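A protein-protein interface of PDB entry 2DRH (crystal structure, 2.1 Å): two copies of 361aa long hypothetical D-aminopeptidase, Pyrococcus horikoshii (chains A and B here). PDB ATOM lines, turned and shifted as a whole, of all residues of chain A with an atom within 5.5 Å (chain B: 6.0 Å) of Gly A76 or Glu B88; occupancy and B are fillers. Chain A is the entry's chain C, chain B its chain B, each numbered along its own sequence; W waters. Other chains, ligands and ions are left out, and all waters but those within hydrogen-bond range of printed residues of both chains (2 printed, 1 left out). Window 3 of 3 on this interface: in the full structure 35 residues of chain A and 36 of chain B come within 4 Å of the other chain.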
ATOM      1  N   VAL A  73     -26.449 -11.452 -17.845  1.00  0.00           N
ATOM      2  CA  VAL A  73     -25.957 -11.988 -19.106  1.00  0.00           C
ATOM      3  C   VAL A  73     -24.512 -12.424 -18.891  1.00  0.00           C
ATOM      4  O   VAL A  73     -23.623 -11.592 -18.739  1.00  0.00           O
ATOM      5  CB  VAL A  73     -26.001 -10.924 -20.228  1.00  0.00           C
ATOM      6  CG1 VAL A  73     -25.354 -11.476 -21.510  1.00  0.00           C
ATOM      7  CG2 VAL A  73     -27.445 -10.519 -20.495  1.00  0.00           C
ATOM      8  N   MET A  74     -24.290 -13.731 -18.839  1.00  0.00           N
ATOM      9  CA  MET A  74     -22.942 -14.250 -18.662  1.00  0.00           C
ATOM     10  C   MET A  74     -22.196 -13.980 -19.979  1.00  0.00           C
ATOM     11  O   MET A  74     -21.128 -13.371 -19.981  1.00  0.00           O
ATOM     12  CB  MET A  74     -22.992 -15.751 -18.349  1.00  0.00           C
ATOM     13  CG  MET A  74     -21.621 -16.388 -18.162  1.00  0.00           C
ATOM     14  SD  MET A  74     -20.591 -15.494 -16.984  1.00  0.00           S
ATOM     15  CE  MET A  74     -19.195 -16.577 -16.918  1.00  0.00           C
ATOM     16  N   ASN A  75     -22.763 -14.432 -21.097  1.00  0.00           N
ATOM     17  CA  ASN A  75     -22.156 -14.171 -22.401  1.00  0.00           C
ATOM     18  C   ASN A  75     -23.245 -13.734 -23.353  1.00  0.00           C
ATOM     19  O   ASN A  75     -24.171 -14.490 -23.636  1.00  0.00           O
ATOM     20  CB  ASN A  75     -21.449 -15.391 -22.978  1.00  0.00           C
ATOM     21  CG  ASN A  75     -20.696 -15.060 -24.272  1.00  0.00           C
ATOM     22  OD1 ASN A  75     -19.922 -14.104 -24.316  1.00  0.00           O
ATOM     23  ND2 ASN A  75     -20.920 -15.850 -25.320  1.00  0.00           N
ATOM     24  N   GLY A  76     -23.113 -12.509 -23.848  1.00  0.00           N
ATOM     25  CA  GLY A  76     -24.107 -11.936 -24.737  1.00  0.00           C
ATOM     26  C   GLY A  76     -24.179 -12.308 -26.210  1.00  0.00           C
ATOM     27  O   GLY A  76     -24.636 -11.496 -27.011  1.00  0.00           O
ATOM     28  N   TYR A  77     -23.732 -13.499 -26.589  1.00  0.00           N
ATOM     29  CA  TYR A  77     -23.854 -13.891 -27.988  1.00  0.00           C
ATOM     30  C   TYR A  77     -25.267 -14.447 -28.015  1.00  0.00           C
ATOM     31  O   TYR A  77     -25.489 -15.637 -28.232  1.00  0.00           O
ATOM     32  CB  TYR A  77     -22.857 -14.986 -28.360  1.00  0.00           C
ATOM     33  CG  TYR A  77     -22.611 -15.061 -29.847  1.00  0.00           C
ATOM     34  CD1 TYR A  77     -21.617 -14.293 -30.443  1.00  0.00           C
ATOM     35  CD2 TYR A  77     -23.407 -15.860 -30.667  1.00  0.00           C
ATOM     36  CE1 TYR A  77     -21.418 -14.315 -31.821  1.00  0.00           C
ATOM     37  CE2 TYR A  77     -23.219 -15.888 -32.046  1.00  0.00           C
ATOM     38  CZ  TYR A  77     -22.222 -15.112 -32.614  1.00  0.00           C
ATOM     39  OH  TYR A  77     -22.041 -15.121 -33.978  1.00  0.00           O
ATOM     40  N   SER A  78     -26.224 -13.561 -27.766  1.00  0.00           N
ATOM     41  CA  SER A  78     -27.621 -13.943 -27.695  1.00  0.00           C
ATOM     42  C   SER A  78     -28.473 -12.815 -28.255  1.00  0.00           C
ATOM     43  O   SER A  78     -28.017 -11.684 -28.370  1.00  0.00           O
ATOM     44  CB  SER A  78     -27.993 -14.212 -26.229  1.00  0.00           C
ATOM     45  OG  SER A  78     -29.261 -14.835 -26.118  1.00  0.00           O
ATOM     46  N   SER A 277     -21.549 -18.971 -27.215  1.00  0.00           N
ATOM     47  CA  SER A 277     -22.598 -19.522 -26.362  1.00  0.00           C
ATOM     48  C   SER A 277     -23.412 -18.440 -25.670  1.00  0.00           C
ATOM     49  O   SER A 277     -22.910 -17.734 -24.803  1.00  0.00           O
ATOM     50  CB  SER A 277     -21.985 -20.452 -25.311  1.00  0.00           C
ATOM     51  OG  SER A 277     -22.971 -21.297 -24.743  1.00  0.00           O
ATOM     52  N   GLY A 278     -24.672 -18.315 -26.059  1.00  0.00           N
ATOM     53  CA  GLY A 278     -25.535 -17.315 -25.457  1.00  0.00           C
ATOM     54  C   GLY A 278     -26.052 -17.791 -24.113  1.00  0.00           C
ATOM     55  O   GLY A 278     -27.048 -18.509 -24.046  1.00  0.00           O
ATOM     56  N   ASP A 279     -25.375 -17.391 -23.042  1.00  0.00           N
ATOM     57  CA  ASP A 279     -25.762 -17.804 -21.702  1.00  0.00           C
ATOM     58  C   ASP A 279     -26.436 -16.663 -20.953  1.00  0.00           C
ATOM     59  O   ASP A 279     -25.807 -15.659 -20.643  1.00  0.00           O
ATOM     60  CB  ASP A 279     -24.537 -18.280 -20.914  1.00  0.00           C
ATOM     61  CG  ASP A 279     -23.761 -19.378 -21.629  1.00  0.00           C
ATOM     62  OD1 ASP A 279     -24.257 -19.943 -22.635  1.00  0.00           O
ATOM     63  OD2 ASP A 279     -22.645 -19.681 -21.168  1.00  0.00           O
ATOM     64  N   LEU B  83     -29.341  -5.213 -28.561  1.00  0.00           N
ATOM     65  CA  LEU B  83     -28.308  -4.489 -27.825  1.00  0.00           C
ATOM     66  C   LEU B  83     -27.364  -5.385 -27.030  1.00  0.00           C
ATOM     67  O   LEU B  83     -26.182  -5.073 -26.867  1.00  0.00           O
ATOM     68  CB  LEU B  83     -28.927  -3.443 -26.887  1.00  0.00           C
ATOM     69  CG  LEU B  83     -29.549  -2.185 -27.507  1.00  0.00           C
ATOM     70  CD1 LEU B  83     -30.041  -1.276 -26.385  1.00  0.00           C
ATOM     71  CD2 LEU B  83     -28.512  -1.443 -28.388  1.00  0.00           C
ATOM     72  N   ILE B  84     -27.880  -6.497 -26.530  1.00  0.00           N
ATOM     73  CA  ILE B  84     -27.068  -7.406 -25.736  1.00  0.00           C
ATOM     74  C   ILE B  84     -25.827  -7.909 -26.493  1.00  0.00           C
ATOM     75  O   ILE B  84     -24.710  -7.868 -25.967  1.00  0.00           O
ATOM     76  CB  ILE B  84     -27.940  -8.581 -25.222  1.00  0.00           C
ATOM     77  CG1 ILE B  84     -28.678  -8.156 -23.938  1.00  0.00           C
ATOM     78  CG2 ILE B  84     -27.081  -9.817 -24.961  1.00  0.00           C
ATOM     79  CD1 ILE B  84     -29.561  -6.906 -24.082  1.00  0.00           C
ATOM     80  N   GLN B  85     -26.003  -8.369 -27.725  1.00  0.00           N
ATOM     81  CA  GLN B  85     -24.850  -8.855 -28.470  1.00  0.00           C
ATOM     82  C   GLN B  85     -23.967  -7.691 -28.876  1.00  0.00           C
ATOM     83  O   GLN B  85     -22.745  -7.826 -28.930  1.00  0.00           O
ATOM     84  CB  GLN B  85     -25.279  -9.652 -29.701  1.00  0.00           C
ATOM     85  CG  GLN B  85     -24.110 -10.336 -30.404  1.00  0.00           C
ATOM     86  CD  GLN B  85     -24.551 -11.498 -31.269  1.00  0.00           C
ATOM     87  OE1 GLN B  85     -25.320 -12.348 -30.823  1.00  0.00           O
ATOM     88  NE2 GLN B  85     -24.055 -11.551 -32.505  1.00  0.00           N
ATOM     89  N   LEU B  86     -24.586  -6.542 -29.142  1.00  0.00           N
ATOM     90  CA  LEU B  86     -23.846  -5.353 -29.521  1.00  0.00           C
ATOM     91  C   LEU B  86     -22.850  -5.031 -28.410  1.00  0.00           C
ATOM     92  O   LEU B  86     -21.680  -4.740 -28.685  1.00  0.00           O
ATOM     93  CB  LEU B  86     -24.804  -4.177 -29.755  1.00  0.00           C
ATOM     94  CG  LEU B  86     -24.227  -2.868 -30.313  1.00  0.00           C
ATOM     95  CD1 LEU B  86     -25.355  -1.949 -30.747  1.00  0.00           C
ATOM     96  CD2 LEU B  86     -23.348  -2.193 -29.278  1.00  0.00           C
ATOM     97  N   TRP B  87     -23.300  -5.093 -27.156  1.00  0.00           N
ATOM     98  CA  TRP B  87     -22.402  -4.813 -26.036  1.00  0.00           C
ATOM     99  C   TRP B  87     -21.357  -5.910 -25.837  1.00  0.00           C
ATOM    100  O   TRP B  87     -20.186  -5.624 -25.553  1.00  0.00           O
ATOM    101  CB  TRP B  87     -23.176  -4.631 -24.720  1.00  0.00           C
ATOM    102  CG  TRP B  87     -23.897  -3.313 -24.601  1.00  0.00           C
ATOM    103  CD1 TRP B  87     -23.403  -2.074 -24.912  1.00  0.00           C
ATOM    104  CD2 TRP B  87     -25.219  -3.097 -24.082  1.00  0.00           C
ATOM    105  NE1 TRP B  87     -24.331  -1.105 -24.618  1.00  0.00           N
ATOM    106  CE2 TRP B  87     -25.453  -1.701 -24.106  1.00  0.00           C
ATOM    107  CE3 TRP B  87     -26.225  -3.944 -23.596  1.00  0.00           C
ATOM    108  CZ2 TRP B  87     -26.658  -1.131 -23.663  1.00  0.00           C
ATOM    109  CZ3 TRP B  87     -27.428  -3.374 -23.153  1.00  0.00           C
ATOM    110  CH2 TRP B  87     -27.629  -1.982 -23.192  1.00  0.00           C
ATOM    111  N   GLU B  88     -21.779  -7.163 -25.975  1.00  0.00           N
ATOM    112  CA  GLU B  88     -20.870  -8.281 -25.779  1.00  0.00           C
ATOM    113  C   GLU B  88     -19.750  -8.338 -26.823  1.00  0.00           C
ATOM    114  O   GLU B  88     -18.587  -8.506 -26.470  1.00  0.00           O
ATOM    115  CB  GLU B  88     -21.639  -9.606 -25.807  1.00  0.00           C
ATOM    116  CG  GLU B  88     -20.806 -10.831 -25.424  1.00  0.00           C
ATOM    117  CD  GLU B  88     -20.501 -10.884 -23.932  1.00  0.00           C
ATOM    118  OE1 GLU B  88     -21.470 -10.881 -23.129  1.00  0.00           O
ATOM    119  OE2 GLU B  88     -19.301 -10.933 -23.559  1.00  0.00           O
ATOM    120  N   LEU B  89     -20.110  -8.182 -28.096  1.00  0.00           N
ATOM    121  CA  LEU B  89     -19.154  -8.273 -29.199  1.00  0.00           C
ATOM    122  C   LEU B  89     -18.631  -6.960 -29.754  1.00  0.00           C
ATOM    123  O   LEU B  89     -17.679  -6.956 -30.540  1.00  0.00           O
ATOM    124  CB  LEU B  89     -19.767  -9.064 -30.352  1.00  0.00           C
ATOM    125  CG  LEU B  89     -20.320 -10.449 -30.038  1.00  0.00           C
ATOM    126  CD1 LEU B  89     -20.634 -11.143 -31.357  1.00  0.00           C
ATOM    127  CD2 LEU B  89     -19.315 -11.255 -29.240  1.00  0.00           C
ATOM    128  N   GLY B  90     -19.265  -5.856 -29.365  1.00  0.00           N
ATOM    129  CA  GLY B  90     -18.838  -4.549 -29.829  1.00  0.00           C
ATOM    130  C   GLY B  90     -19.096  -4.301 -31.303  1.00  0.00           C
ATOM    131  O   GLY B  90     -18.462  -3.435 -31.914  1.00  0.00           O
HETATM  132  O   HOH W   1     -28.710  -8.960 -28.953  1.00  0.00           O
HETATM  133  O   HOH W   2     -24.903 -13.341 -34.451  1.00  0.00           O
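N of Gln B85 lies close to O of Gly A76 (3.5 Å). The side-chain amide oxygen of Gln B85 lies within hydrogen-bond range of the backbone NH of Ser A78, 3.4 Å away. The side-chain amide oxygen of Asn A75 sits close to the side-chain carboxylate of Glu B88, at 3.3 Å. The side-chain carboxylate of Glu B88 lies within hydrogen-bond range of the backbone NH of Gly A76.
The side-chain amide nitrogen of Asn A75 sits at hydrogen-bond distance from the backbone carbonyl oxygen of Ser A277. O of Asn A75 is in hydrogen-bond range of N of Asp A279 (3.2 Å).
Gly A76 touches Ile B84. Tyr A77 touches Gln B85 (C to OE1, 3.5 Å). CE1 of Tyr A77 touches CD1 of Leu B89 (3.3 Å). Ser A78 touches Ile B84.
Met A74 touches none of the printed residues of chain B. Printed residues of chain B within 4 Å of Asn A75: Glu B88. Gly A76 touches three residues of chain B. Of the printed residues of chain B, Tyr A77 touches Gln B85 (3.5 Å) and Leu B89 (3.3 Å). Of the printed residues of chain B, Ser A78 touches Ile B84 (3.998 Å) and Gln B85 (3.4 Å). Of the printed residues of chain A, Ile B84 touches Gly A76 (3.6 Å) and Ser A78 (3.998 Å). Of the printed residues of chain A, Gln B85 touches Gly A76 (3.0 Å), Tyr A77 (3.5 Å) and Ser A78 (3.4 Å). The nearest printed residue of chain B that does not touch Gly A76 is Leu B89 (5.4 Å).
Printed residues of chain B that touch a printed residue of chain A: Ile B84, Gln B85, Glu B88 and Leu B89. Hydrophobic or aromatic side chains of chain B within 4 Å of the printed part of chain A: Ile B84 and Leu B89. Of the 9 printed residues of chain A, 4 touch a printed residue of chain B. Hydrophobic or aromatic side chains of chain A within 4 Å of the printed part of chain B: Tyr A77. Among the printed residues, 8 pairs touch across the chains. Among the printed residues, no Asp or Glu carboxylate lies within 4 Å of a Lys or Arg side-chain nitrogen of the other chain.
No position is printed for both chains. Of the 8 pairs that touch across the chains among the printed residues, none has its exchanged pair printed and touching as well.
Water W2 bridges the side-chain amide nitrogen of Gln B85 (2.8 Å) and the side-chain hydroxyl of Tyr A77 (3.4 Å). Water W1 bridges O of Ser A78 (2.9 Å) and N of Gln B85 (3.0 Å).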
